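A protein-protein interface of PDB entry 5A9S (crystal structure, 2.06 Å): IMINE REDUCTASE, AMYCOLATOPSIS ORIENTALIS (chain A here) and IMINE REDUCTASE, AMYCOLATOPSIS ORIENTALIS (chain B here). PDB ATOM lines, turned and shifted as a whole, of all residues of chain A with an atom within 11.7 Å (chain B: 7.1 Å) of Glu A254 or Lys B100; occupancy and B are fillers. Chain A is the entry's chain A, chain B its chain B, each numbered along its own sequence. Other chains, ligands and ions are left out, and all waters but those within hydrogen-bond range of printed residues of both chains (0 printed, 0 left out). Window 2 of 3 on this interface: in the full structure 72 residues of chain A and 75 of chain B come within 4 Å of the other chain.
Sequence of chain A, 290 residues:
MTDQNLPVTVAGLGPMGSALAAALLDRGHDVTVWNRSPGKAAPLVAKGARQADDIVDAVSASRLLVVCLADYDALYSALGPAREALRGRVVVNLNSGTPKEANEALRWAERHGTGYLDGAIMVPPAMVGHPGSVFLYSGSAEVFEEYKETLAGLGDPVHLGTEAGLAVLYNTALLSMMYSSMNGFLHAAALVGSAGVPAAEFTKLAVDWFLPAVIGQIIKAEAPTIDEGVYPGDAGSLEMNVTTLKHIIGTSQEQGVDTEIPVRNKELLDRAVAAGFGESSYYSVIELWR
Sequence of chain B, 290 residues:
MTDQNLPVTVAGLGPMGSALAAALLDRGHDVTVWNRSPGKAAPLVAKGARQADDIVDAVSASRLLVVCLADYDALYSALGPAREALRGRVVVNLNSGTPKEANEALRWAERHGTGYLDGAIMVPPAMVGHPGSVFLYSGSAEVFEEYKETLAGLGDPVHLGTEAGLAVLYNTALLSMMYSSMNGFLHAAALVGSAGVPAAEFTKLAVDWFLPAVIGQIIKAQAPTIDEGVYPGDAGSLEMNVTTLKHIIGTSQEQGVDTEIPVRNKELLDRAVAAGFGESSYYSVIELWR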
ATOM      1  N   HIS A 187     -21.574  -8.647 -27.404  1.00  0.00           N
ATOM      2  CA  HIS A 187     -20.623  -7.695 -26.909  1.00  0.00           C
ATOM      3  C   HIS A 187     -21.274  -6.647 -25.999  1.00  0.00           C
ATOM      4  O   HIS A 187     -20.761  -6.365 -24.896  1.00  0.00           O
ATOM      5  CB  HIS A 187     -19.869  -7.005 -28.020  1.00  0.00           C
ATOM      6  CG  HIS A 187     -18.847  -6.064 -27.495  1.00  0.00           C
ATOM      7  ND1 HIS A 187     -19.001  -4.693 -27.521  1.00  0.00           N
ATOM      8  CD2 HIS A 187     -17.672  -6.310 -26.865  1.00  0.00           C
ATOM      9  CE1 HIS A 187     -17.957  -4.135 -26.926  1.00  0.00           C
ATOM     10  NE2 HIS A 187     -17.130  -5.101 -26.537  1.00  0.00           N
ATOM     11  N   ALA A 190     -22.071  -8.212 -22.668  1.00  0.00           N
ATOM     12  CA  ALA A 190     -20.879  -8.422 -21.896  1.00  0.00           C
ATOM     13  C   ALA A 190     -20.468  -7.144 -21.243  1.00  0.00           C
ATOM     14  O   ALA A 190     -20.110  -7.098 -20.069  1.00  0.00           O
ATOM     15  CB  ALA A 190     -19.762  -8.940 -22.779  1.00  0.00           C
ATOM     16  N   LEU A 191     -20.559  -6.078 -22.012  1.00  0.00           N
ATOM     17  CA  LEU A 191     -20.262  -4.752 -21.528  1.00  0.00           C
ATOM     18  C   LEU A 191     -21.113  -4.283 -20.391  1.00  0.00           C
ATOM     19  O   LEU A 191     -20.581  -3.865 -19.383  1.00  0.00           O
ATOM     20  CB  LEU A 191     -20.346  -3.775 -22.660  1.00  0.00           C
ATOM     21  CG  LEU A 191     -19.593  -2.471 -22.571  1.00  0.00           C
ATOM     22  CD1 LEU A 191     -18.106  -2.636 -22.266  1.00  0.00           C
ATOM     23  CD2 LEU A 191     -19.814  -1.665 -23.853  1.00  0.00           C
ATOM     24  N   VAL A 192     -22.431  -4.365 -20.491  1.00  0.00           N
ATOM     25  CA  VAL A 192     -23.232  -3.946 -19.352  1.00  0.00           C
ATOM     26  C   VAL A 192     -23.088  -4.922 -18.189  1.00  0.00           C
ATOM     27  O   VAL A 192     -23.152  -4.525 -16.997  1.00  0.00           O
ATOM     28  CB  VAL A 192     -24.733  -3.710 -19.674  1.00  0.00           C
ATOM     29  CG1 VAL A 192     -24.892  -2.648 -20.747  1.00  0.00           C
ATOM     30  CG2 VAL A 192     -25.455  -4.970 -20.080  1.00  0.00           C
ATOM     31  N   GLY A 193     -22.958  -6.198 -18.525  1.00  0.00           N
ATOM     32  CA  GLY A 193     -22.753  -7.233 -17.519  1.00  0.00           C
ATOM     33  C   GLY A 193     -21.509  -7.010 -16.656  1.00  0.00           C
ATOM     34  O   GLY A 193     -21.524  -7.320 -15.481  1.00  0.00           O
ATOM     35  N   SER A 194     -20.461  -6.433 -17.222  1.00  0.00           N
ATOM     36  CA  SER A 194     -19.230  -6.156 -16.486  1.00  0.00           C
ATOM     37  C   SER A 194     -19.446  -5.142 -15.363  1.00  0.00           C
ATOM     38  O   SER A 194     -18.650  -5.096 -14.474  1.00  0.00           O
ATOM     39  CB  SER A 194     -18.160  -5.616 -17.441  1.00  0.00           C
ATOM     40  OG  SER A 194     -18.455  -4.269 -17.841  1.00  0.00           O
ATOM     41  N   ALA A 195     -20.494  -4.315 -15.413  1.00  0.00           N
ATOM     42  CA  ALA A 195     -20.846  -3.427 -14.297  1.00  0.00           C
ATOM     43  C   ALA A 195     -21.918  -4.002 -13.423  1.00  0.00           C
ATOM     44  O   ALA A 195     -22.440  -3.306 -12.556  1.00  0.00           O
ATOM     45  CB  ALA A 195     -21.355  -2.089 -14.821  1.00  0.00           C
ATOM     46  N   GLY A 196     -22.335  -5.243 -13.681  1.00  0.00           N
ATOM     47  CA  GLY A 196     -23.360  -5.884 -12.879  1.00  0.00           C
ATOM     48  C   GLY A 196     -24.776  -5.564 -13.267  1.00  0.00           C
ATOM     49  O   GLY A 196     -25.696  -5.774 -12.459  1.00  0.00           O
ATOM     50  N   THR A 244     -16.780   7.564 -32.441  1.00  0.00           N
ATOM     51  CA  THR A 244     -17.696   6.851 -31.587  1.00  0.00           C
ATOM     52  C   THR A 244     -17.138   5.455 -31.274  1.00  0.00           C
ATOM     53  O   THR A 244     -17.109   5.042 -30.130  1.00  0.00           O
ATOM     54  CB  THR A 244     -19.090   6.760 -32.221  1.00  0.00           C
ATOM     55  OG1 THR A 244     -19.565   8.096 -32.453  1.00  0.00           O
ATOM     56  CG2 THR A 244     -20.075   6.005 -31.359  1.00  0.00           C
ATOM     57  N   LEU A 245     -16.658   4.750 -32.279  1.00  0.00           N
ATOM     58  CA  LEU A 245     -16.082   3.441 -32.047  1.00  0.00           C
ATOM     59  C   LEU A 245     -14.871   3.457 -31.079  1.00  0.00           C
ATOM     60  O   LEU A 245     -14.697   2.525 -30.272  1.00  0.00           O
ATOM     61  CB  LEU A 245     -15.743   2.789 -33.379  1.00  0.00           C
ATOM     62  CG  LEU A 245     -16.967   1.970 -33.917  1.00  0.00           C
ATOM     63  CD1 LEU A 245     -16.812   1.766 -35.415  1.00  0.00           C
ATOM     64  CD2 LEU A 245     -17.193   0.621 -33.258  1.00  0.00           C
ATOM     65  N   LYS A 246     -14.056   4.512 -31.145  1.00  0.00           N
ATOM     66  CA  LYS A 246     -12.908   4.681 -30.197  1.00  0.00           C
ATOM     67  C   LYS A 246     -13.377   4.823 -28.739  1.00  0.00           C
ATOM     68  O   LYS A 246     -12.777   4.257 -27.850  1.00  0.00           O
ATOM     69  CB  LYS A 246     -12.041   5.881 -30.561  1.00  0.00           C
ATOM     70  CG  LYS A 246     -11.178   5.694 -31.809  1.00  0.00           C
ATOM     71  CD  LYS A 246     -10.370   6.980 -32.054  1.00  0.00           C
ATOM     72  CE  LYS A 246      -9.374   6.884 -33.215  1.00  0.00           C
ATOM     73  NZ  LYS A 246      -9.209   8.215 -33.888  1.00  0.00           N
ATOM     74  N   HIS A 247     -14.481   5.525 -28.520  1.00  0.00           N
ATOM     75  CA  HIS A 247     -15.090   5.560 -27.188  1.00  0.00           C
ATOM     76  C   HIS A 247     -15.568   4.179 -26.710  1.00  0.00           C
ATOM     77  O   HIS A 247     -15.514   3.887 -25.528  1.00  0.00           O
ATOM     78  CB  HIS A 247     -16.267   6.546 -27.181  1.00  0.00           C
ATOM     79  CG  HIS A 247     -15.848   7.980 -27.323  1.00  0.00           C
ATOM     80  ND1 HIS A 247     -16.678   8.964 -27.820  1.00  0.00           N
ATOM     81  CD2 HIS A 247     -14.669   8.591 -27.056  1.00  0.00           C
ATOM     82  CE1 HIS A 247     -16.032  10.118 -27.842  1.00  0.00           C
ATOM     83  NE2 HIS A 247     -14.811   9.915 -27.388  1.00  0.00           N
ATOM     84  N   ILE A 248     -16.159   3.400 -27.624  1.00  0.00           N
ATOM     85  CA  ILE A 248     -16.694   2.072 -27.314  1.00  0.00           C
ATOM     86  C   ILE A 248     -15.500   1.187 -26.971  1.00  0.00           C
ATOM     87  O   ILE A 248     -15.515   0.508 -25.973  1.00  0.00           O
ATOM     88  CB  ILE A 248     -17.486   1.479 -28.492  1.00  0.00           C
ATOM     89  CG1 ILE A 248     -18.776   2.260 -28.722  1.00  0.00           C
ATOM     90  CG2 ILE A 248     -17.850   0.007 -28.253  1.00  0.00           C
ATOM     91  CD1 ILE A 248     -19.408   1.954 -30.081  1.00  0.00           C
ATOM     92  N   ILE A 249     -14.438   1.263 -27.751  1.00  0.00           N
ATOM     93  CA  ILE A 249     -13.239   0.494 -27.424  1.00  0.00           C
ATOM     94  C   ILE A 249     -12.704   0.925 -26.042  1.00  0.00           C
ATOM     95  O   ILE A 249     -12.405   0.074 -25.208  1.00  0.00           O
ATOM     96  CB  ILE A 249     -12.175   0.668 -28.520  1.00  0.00           C
ATOM     97  CG1 ILE A 249     -12.657  -0.042 -29.804  1.00  0.00           C
ATOM     98  CG2 ILE A 249     -10.822   0.131 -28.087  1.00  0.00           C
ATOM     99  CD1 ILE A 249     -11.937   0.390 -31.043  1.00  0.00           C
ATOM    100  N   GLY A 250     -12.612   2.225 -25.812  1.00  0.00           N
ATOM    101  CA  GLY A 250     -12.100   2.778 -24.520  1.00  0.00           C
ATOM    102  C   GLY A 250     -12.925   2.299 -23.339  1.00  0.00           C
ATOM    103  O   GLY A 250     -12.401   1.893 -22.319  1.00  0.00           O
ATOM    104  N   THR A 251     -14.252   2.291 -23.511  1.00  0.00           N
ATOM    105  CA  THR A 251     -15.148   1.880 -22.473  1.00  0.00           C
ATOM    106  C   THR A 251     -15.008   0.378 -22.267  1.00  0.00           C
ATOM    107  O   THR A 251     -15.041  -0.091 -21.147  1.00  0.00           O
ATOM    108  CB  THR A 251     -16.594   2.249 -22.839  1.00  0.00           C
ATOM    109  OG1 THR A 251     -16.717   3.677 -22.920  1.00  0.00           O
ATOM    110  CG2 THR A 251     -17.583   1.652 -21.875  1.00  0.00           C
ATOM    111  N   SER A 252     -14.880  -0.385 -23.338  1.00  0.00           N
ATOM    112  CA  SER A 252     -14.667  -1.812 -23.229  1.00  0.00           C
ATOM    113  C   SER A 252     -13.350  -2.137 -22.449  1.00  0.00           C
ATOM    114  O   SER A 252     -13.340  -2.998 -21.565  1.00  0.00           O
ATOM    115  CB  SER A 252     -14.749  -2.455 -24.675  1.00  0.00           C
ATOM    116  OG  SER A 252     -14.795  -3.846 -24.598  1.00  0.00           O
ATOM    117  N   GLN A 253     -12.266  -1.461 -22.795  1.00  0.00           N
ATOM    118  CA  GLN A 253     -10.993  -1.556 -22.036  1.00  0.00           C
ATOM    119  C   GLN A 253     -11.167  -1.192 -20.544  1.00  0.00           C
ATOM    120  O   GLN A 253     -10.819  -1.990 -19.698  1.00  0.00           O
ATOM    121  CB  GLN A 253      -9.925  -0.651 -22.634  1.00  0.00           C
ATOM    122  CG  GLN A 253      -9.383  -1.183 -23.933  1.00  0.00           C
ATOM    123  CD  GLN A 253      -8.580  -0.159 -24.717  1.00  0.00           C
ATOM    124  OE1 GLN A 253      -8.533   1.018 -24.376  1.00  0.00           O
ATOM    125  NE2 GLN A 253      -7.928  -0.614 -25.782  1.00  0.00           N
ATOM    126  N   GLU A 254     -11.800  -0.064 -20.221  1.00  0.00           N
ATOM    127  CA  GLU A 254     -12.018   0.254 -18.794  1.00  0.00           C
ATOM    128  C   GLU A 254     -12.869  -0.768 -18.074  1.00  0.00           C
ATOM    129  O   GLU A 254     -12.683  -0.967 -16.891  1.00  0.00           O
ATOM    130  CB  GLU A 254     -12.752   1.581 -18.534  1.00  0.00           C
ATOM    131  CG  GLU A 254     -12.163   2.841 -19.077  1.00  0.00           C
ATOM    132  CD  GLU A 254     -13.100   4.093 -18.959  1.00  0.00           C
ATOM    133  OE1 GLU A 254     -14.190   4.054 -18.309  1.00  0.00           O
ATOM    134  OE2 GLU A 254     -12.778   5.119 -19.595  1.00  0.00           O
ATOM    135  N   GLN A 255     -13.824  -1.385 -18.772  1.00  0.00           N
ATOM    136  CA  GLN A 255     -14.662  -2.399 -18.158  1.00  0.00           C
ATOM    137  C   GLN A 255     -14.061  -3.802 -18.129  1.00  0.00           C
ATOM    138  O   GLN A 255     -14.679  -4.695 -17.571  1.00  0.00           O
ATOM    139  CB  GLN A 255     -16.032  -2.458 -18.859  1.00  0.00           C
ATOM    140  CG  GLN A 255     -16.835  -1.173 -18.722  1.00  0.00           C
ATOM    141  CD  GLN A 255     -17.145  -0.808 -17.269  1.00  0.00           C
ATOM    142  OE1 GLN A 255     -16.856   0.289 -16.849  1.00  0.00           O
ATOM    143  NE2 GLN A 255     -17.735  -1.733 -16.509  1.00  0.00           N
ATOM    144  N   GLY A 256     -12.906  -4.013 -18.740  1.00  0.00           N
ATOM    145  CA  GLY A 256     -12.303  -5.336 -18.754  1.00  0.00           C
ATOM    146  C   GLY A 256     -12.984  -6.286 -19.729  1.00  0.00           C
ATOM    147  O   GLY A 256     -12.897  -7.476 -19.551  1.00  0.00           O
ATOM    148  N   VAL A 257     -13.630  -5.780 -20.780  1.00  0.00           N
ATOM    149  CA  VAL A 257     -14.319  -6.633 -21.745  1.00  0.00           C
ATOM    150  C   VAL A 257     -13.512  -6.649 -23.019  1.00  0.00           C
ATOM    151  O   VAL A 257     -13.026  -5.625 -23.425  1.00  0.00           O
ATOM    152  CB  VAL A 257     -15.752  -6.161 -21.944  1.00  0.00           C
ATOM    153  CG1 VAL A 257     -16.431  -6.881 -23.112  1.00  0.00           C
ATOM    154  CG2 VAL A 257     -16.508  -6.401 -20.647  1.00  0.00           C
ATOM    155  N   ASP A 258     -13.369  -7.820 -23.626  1.00  0.00           N
ATOM    156  CA  ASP A 258     -12.580  -7.995 -24.841  1.00  0.00           C
ATOM    157  C   ASP A 258     -13.044  -7.030 -25.930  1.00  0.00           C
ATOM    158  O   ASP A 258     -14.245  -6.826 -26.146  1.00  0.00           O
ATOM    159  CB  ASP A 258     -12.653  -9.451 -25.309  1.00  0.00           C
ATOM    160  CG  ASP A 258     -11.651  -9.821 -26.375  1.00  0.00           C
ATOM    161  OD1 ASP A 258     -11.449  -9.133 -27.393  1.00  0.00           O
ATOM    162  OD2 ASP A 258     -11.098 -10.913 -26.245  1.00  0.00           O
ATOM    163  N   THR A 259     -12.110  -6.372 -26.560  1.00  0.00           N
ATOM    164  CA  THR A 259     -12.456  -5.372 -27.537  1.00  0.00           C
ATOM    165  C   THR A 259     -12.546  -5.811 -28.977  1.00  0.00           C
ATOM    166  O   THR A 259     -12.745  -5.019 -29.837  1.00  0.00           O
ATOM    167  CB  THR A 259     -11.473  -4.225 -27.481  1.00  0.00           C
ATOM    168  OG1 THR A 259     -10.182  -4.746 -27.686  1.00  0.00           O
ATOM    169  CG2 THR A 259     -11.497  -3.592 -26.161  1.00  0.00           C
ATOM    170  N   GLU A 260     -12.389  -7.094 -29.210  1.00  0.00           N
ATOM    171  CA  GLU A 260     -12.441  -7.655 -30.565  1.00  0.00           C
ATOM    172  C   GLU A 260     -13.542  -7.095 -31.483  1.00  0.00           C
ATOM    173  O   GLU A 260     -13.288  -6.643 -32.627  1.00  0.00           O
ATOM    174  CB  GLU A 260     -12.601  -9.167 -30.413  1.00  0.00           C
ATOM    175  CG  GLU A 260     -12.968  -9.922 -31.667  1.00  0.00           C
ATOM    176  CD  GLU A 260     -12.950 -11.420 -31.525  1.00  0.00           C
ATOM    177  OE1 GLU A 260     -12.986 -12.007 -30.427  1.00  0.00           O
ATOM    178  OE2 GLU A 260     -12.933 -12.032 -32.589  1.00  0.00           O
ATOM    179  N   PRO A 262     -15.628  -4.356 -31.256  1.00  0.00           N
ATOM    180  CA  PRO A 262     -15.571  -2.956 -31.711  1.00  0.00           C
ATOM    181  C   PRO A 262     -14.260  -2.587 -32.424  1.00  0.00           C
ATOM    182  O   PRO A 262     -14.259  -1.720 -33.309  1.00  0.00           O
ATOM    183  CB  PRO A 262     -15.765  -2.154 -30.415  1.00  0.00           C
ATOM    184  CG  PRO A 262     -15.357  -3.070 -29.366  1.00  0.00           C
ATOM    185  CD  PRO A 262     -15.779  -4.448 -29.800  1.00  0.00           C
ATOM    186  N   VAL A 263     -13.166  -3.286 -32.088  1.00  0.00           N
ATOM    187  CA  VAL A 263     -11.905  -3.126 -32.875  1.00  0.00           C
ATOM    188  C   VAL A 263     -12.107  -3.511 -34.335  1.00  0.00           C
ATOM    189  O   VAL A 263     -11.739  -2.744 -35.225  1.00  0.00           O
ATOM    190  CB  VAL A 263     -10.718  -3.858 -32.222  1.00  0.00           C
ATOM    191  CG1 VAL A 263      -9.517  -3.956 -33.178  1.00  0.00           C
ATOM    192  CG2 VAL A 263     -10.329  -3.113 -30.943  1.00  0.00           C
ATOM    193  N   TYR B  76     -14.586  21.009 -17.824  1.00  0.00           N
ATOM    194  CA  TYR B  76     -13.891  21.570 -16.678  1.00  0.00           C
ATOM    195  C   TYR B  76     -13.361  22.957 -17.039  1.00  0.00           C
ATOM    196  O   TYR B  76     -13.359  23.879 -16.227  1.00  0.00           O
ATOM    197  CB  TYR B  76     -12.792  20.590 -16.210  1.00  0.00           C
ATOM    198  CG  TYR B  76     -13.299  19.107 -16.181  1.00  0.00           C
ATOM    199  CD1 TYR B  76     -14.474  18.762 -15.531  1.00  0.00           C
ATOM    200  CD2 TYR B  76     -12.619  18.084 -16.845  1.00  0.00           C
ATOM    201  CE1 TYR B  76     -14.958  17.444 -15.529  1.00  0.00           C
ATOM    202  CE2 TYR B  76     -13.099  16.764 -16.833  1.00  0.00           C
ATOM    203  CZ  TYR B  76     -14.279  16.457 -16.175  1.00  0.00           C
ATOM    204  OH  TYR B  76     -14.786  15.159 -16.147  1.00  0.00           O
ATOM    205  N   GLY B  97     -17.709  10.539 -22.908  1.00  0.00           N
ATOM    206  CA  GLY B  97     -17.164   9.500 -23.720  1.00  0.00           C
ATOM    207  C   GLY B  97     -17.193   8.151 -23.064  1.00  0.00           C
ATOM    208  O   GLY B  97     -17.667   7.246 -23.663  1.00  0.00           O
ATOM    209  N   THR B  98     -16.683   8.021 -21.853  1.00  0.00           N
ATOM    210  CA  THR B  98     -16.653   6.749 -21.155  1.00  0.00           C
ATOM    211  C   THR B  98     -17.223   6.861 -19.751  1.00  0.00           C
ATOM    212  O   THR B  98     -17.390   7.938 -19.269  1.00  0.00           O
ATOM    213  CB  THR B  98     -15.220   6.234 -21.015  1.00  0.00           C
ATOM    214  OG1 THR B  98     -14.539   6.992 -20.042  1.00  0.00           O
ATOM    215  CG2 THR B  98     -14.488   6.378 -22.246  1.00  0.00           C
ATOM    216  N   PRO B  99     -17.501   5.737 -19.095  1.00  0.00           N
ATOM    217  CA  PRO B  99     -18.008   5.820 -17.742  1.00  0.00           C
ATOM    218  C   PRO B  99     -17.075   6.476 -16.734  1.00  0.00           C
ATOM    219  O   PRO B  99     -17.546   7.200 -15.892  1.00  0.00           O
ATOM    220  CB  PRO B  99     -18.265   4.351 -17.370  1.00  0.00           C
ATOM    221  CG  PRO B  99     -18.509   3.679 -18.673  1.00  0.00           C
ATOM    222  CD  PRO B  99     -17.591   4.360 -19.634  1.00  0.00           C
ATOM    223  N   LYS B 100     -15.774   6.187 -16.794  1.00  0.00           N
ATOM    224  CA  LYS B 100     -14.806   6.895 -15.982  1.00  0.00           C
ATOM    225  C   LYS B 100     -14.936   8.439 -16.173  1.00  0.00           C
ATOM    226  O   LYS B 100     -14.958   9.141 -15.197  1.00  0.00           O
ATOM    227  CB  LYS B 100     -13.371   6.455 -16.289  1.00  0.00           C
ATOM    228  N   GLU B 101     -15.064   8.932 -17.409  1.00  0.00           N
ATOM    229  CA  GLU B 101     -15.259  10.383 -17.622  1.00  0.00           C
ATOM    230  C   GLU B 101     -16.560  10.909 -17.017  1.00  0.00           C
ATOM    231  O   GLU B 101     -16.558  11.973 -16.420  1.00  0.00           O
ATOM    232  CB  GLU B 101     -15.244  10.765 -19.074  1.00  0.00           C
ATOM    233  CG  GLU B 101     -13.938  10.466 -19.763  1.00  0.00           C
ATOM    234  CD  GLU B 101     -14.089  10.608 -21.250  1.00  0.00           C
ATOM    235  OE1 GLU B 101     -14.720  11.592 -21.676  1.00  0.00           O
ATOM    236  OE2 GLU B 101     -13.665   9.689 -21.982  1.00  0.00           O
ATOM    237  N   ALA B 102     -17.644  10.141 -17.105  1.00  0.00           N
ATOM    238  CA  ALA B 102     -18.871  10.511 -16.409  1.00  0.00           C
ATOM    239  C   ALA B 102     -18.661  10.623 -14.913  1.00  0.00           C
ATOM    240  O   ALA B 102     -19.186  11.558 -14.270  1.00  0.00           O
ATOM    241  CB  ALA B 102     -19.989   9.542 -16.718  1.00  0.00           C
ATOM    242  N   ASN B 103     -17.928   9.665 -14.356  1.00  0.00           N
ATOM    243  CA  ASN B 103     -17.611   9.691 -12.932  1.00  0.00           C
ATOM    244  C   ASN B 103     -16.725  10.853 -12.494  1.00  0.00           C
ATOM    245  O   ASN B 103     -16.955  11.437 -11.446  1.00  0.00           O
ATOM    246  CB  ASN B 103     -16.955   8.380 -12.494  1.00  0.00           C
ATOM    247  CG  ASN B 103     -17.939   7.381 -12.060  1.00  0.00           C
ATOM    248  OD1 ASN B 103     -18.141   7.241 -10.866  1.00  0.00           O
ATOM    249  ND2 ASN B 103     -18.562   6.715 -12.951  1.00  0.00           N
ATOM    250  N   GLU B 104     -15.740  11.185 -13.303  1.00  0.00           N
ATOM    251  CA  GLU B 104     -14.920  12.386 -13.059  1.00  0.00           C
ATOM    252  C   GLU B 104     -15.782  13.654 -13.100  1.00  0.00           C
ATOM    253  O   GLU B 104     -15.580  14.562 -12.325  1.00  0.00           O
ATOM    254  CB  GLU B 104     -13.805  12.524 -14.094  1.00  0.00           C
ATOM    255  CG  GLU B 104     -12.586  11.652 -13.833  1.00  0.00           C
ATOM    256  CD  GLU B 104     -11.752  11.368 -15.103  1.00  0.00           C
ATOM    257  OE1 GLU B 104     -11.654  12.267 -15.952  1.00  0.00           O
ATOM    258  OE2 GLU B 104     -11.185  10.260 -15.255  1.00  0.00           O
ATOM    259  N   ALA B 105     -16.724  13.730 -14.024  1.00  0.00           N
ATOM    260  CA  ALA B 105     -17.581  14.939 -14.128  1.00  0.00           C
ATOM    261  C   ALA B 105     -18.483  15.038 -12.910  1.00  0.00           C
ATOM    262  O   ALA B 105     -18.652  16.114 -12.346  1.00  0.00           O
ATOM    263  CB  ALA B 105     -18.390  14.922 -15.399  1.00  0.00           C
ATOM    264  N   LEU B 106     -19.045  13.923 -12.477  1.00  0.00           N
ATOM    265  CA  LEU B 106     -19.809  13.889 -11.214  1.00  0.00           C
ATOM    266  C   LEU B 106     -18.986  14.441 -10.054  1.00  0.00           C
ATOM    267  O   LEU B 106     -19.500  15.242  -9.275  1.00  0.00           O
ATOM    268  CB  LEU B 106     -20.194  12.462 -10.883  1.00  0.00           C
ATOM    269  CG  LEU B 106     -21.183  12.020  -9.802  1.00  0.00           C
ATOM    270  CD1 LEU B 106     -20.625  11.179  -8.697  1.00  0.00           C
ATOM    271  CD2 LEU B 106     -22.209  13.020  -9.322  1.00  0.00           C
ATOM    272  N   ARG B 107     -17.739  13.984  -9.908  1.00  0.00           N
ATOM    273  CA  ARG B 107     -16.884  14.462  -8.776  1.00  0.00           C
ATOM    274  C   ARG B 107     -16.667  15.923  -8.879  1.00  0.00           C
ATOM    275  O   ARG B 107     -16.792  16.622  -7.931  1.00  0.00           O
ATOM    276  CB  ARG B 107     -15.503  13.805  -8.746  1.00  0.00           C
ATOM    277  CG  ARG B 107     -15.586  12.480  -8.024  1.00  0.00           C
ATOM    278  CD  ARG B 107     -14.348  11.617  -8.127  1.00  0.00           C
ATOM    279  NE  ARG B 107     -14.808  10.240  -8.269  1.00  0.00           N
ATOM    280  CZ  ARG B 107     -14.644   9.462  -9.339  1.00  0.00           C
ATOM    281  NH1 ARG B 107     -13.927   9.848 -10.412  1.00  0.00           N
ATOM    282  NH2 ARG B 107     -15.191   8.256  -9.322  1.00  0.00           N
ATOM    283  N   GLY B 165     -22.100   6.804 -14.353  1.00  0.00           N
ATOM    284  CA  GLY B 165     -21.588   6.160 -15.528  1.00  0.00           C
ATOM    285  C   GLY B 165     -22.526   5.272 -16.320  1.00  0.00           C
ATOM    286  O   GLY B 165     -22.181   4.852 -17.387  1.00  0.00           O
ATOM    287  N   VAL B 168     -23.719   6.383 -20.308  1.00  0.00           N
ATOM    288  CA  VAL B 168     -22.642   6.138 -21.262  1.00  0.00           C
ATOM    289  C   VAL B 168     -22.326   4.671 -21.426  1.00  0.00           C
ATOM    290  O   VAL B 168     -22.025   4.210 -22.535  1.00  0.00           O
ATOM    291  CB  VAL B 168     -21.378   6.911 -20.856  1.00  0.00           C
ATOM    292  CG1 VAL B 168     -20.210   6.638 -21.810  1.00  0.00           C
ATOM    293  CG2 VAL B 168     -21.738   8.378 -20.991  1.00  0.00           C
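OE2 of Glu A254 lies within hydrogen-bond range of OG1 of Thr B98.
The backbone NH (N) of Lys B100 lies within hydrogen-bond range of the side-chain carboxylate (OE1) of Glu A254, at 3.1 Å.
Of the 14 printed residues of chain B, 4 touch a printed residue of chain A.
Hydrophobic or aromatic side chains of chain B that line the printed part of chain A: Pro B99.
Along chain B the printed residues that touch a printed residue of chain A span positions 97 to 100.
Of the 27 printed residues of chain A, 3 touch a printed residue of chain B.
Printed residues of chain A that touch a printed residue of chain B: His A247, Thr A251 and Glu A254.
OG1 of Thr B98 lies within hydrogen-bond range of N of Glu B101 (3.3 Å).
OG1 of Thr A251 sits at hydrogen-bond distance from O of His A247 (2.9 Å).
The side-chain amide nitrogen (ND2) of Asn B103 sits at hydrogen-bond distance from the backbone carbonyl oxygen (O) of Pro B99 (3.1 Å).
OE1 of Glu B101 lies within hydrogen-bond range of N of Gly B97 (3.4 Å).
Among the printed residues, pairs that only touch across the chains: Thr A251 with Pro B99 (3.5 Å), Thr A251 with Thr B98 (3.5 Å), Glu A254 with Pro B99 (3.7 Å), Thr A251 with Gly B97 (3.8 Å) and His A247 with Gly B97 (3.9 Å).
Glu A254 touches just these residues of chain B: Thr B98 (2.6 Å), Pro B99 (3.7 Å) and Lys B100 (3.1 Å).
Printed residues of chain A within 4 Å of Lys B100: Glu A254 (3.1 Å).
Of chain A, only His A247 (3.9 Å) and Thr A251 (3.8 Å) come within 4 Å of Gly B97.
Thr B98 touches just these residues of chain A: Thr A251 and Glu A254.
No residue of chain A comes within 4 Å of Glu B101.
No residue of chain A comes within 4 Å of Ala B102.
No residue of chain A comes within 4 Å of Gly B165.
Of the printed residues of chain B, Thr A251 touches Gly B97, Thr B98 and Pro B99.
Of the printed residues of chain B, His A247 touches Gly B97 (3.9 Å).
Thr A244 touches none of the printed residues of chain B.
The nearest printed residue of chain B that does not touch Thr A251 is Val B168 (4.7 Å).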
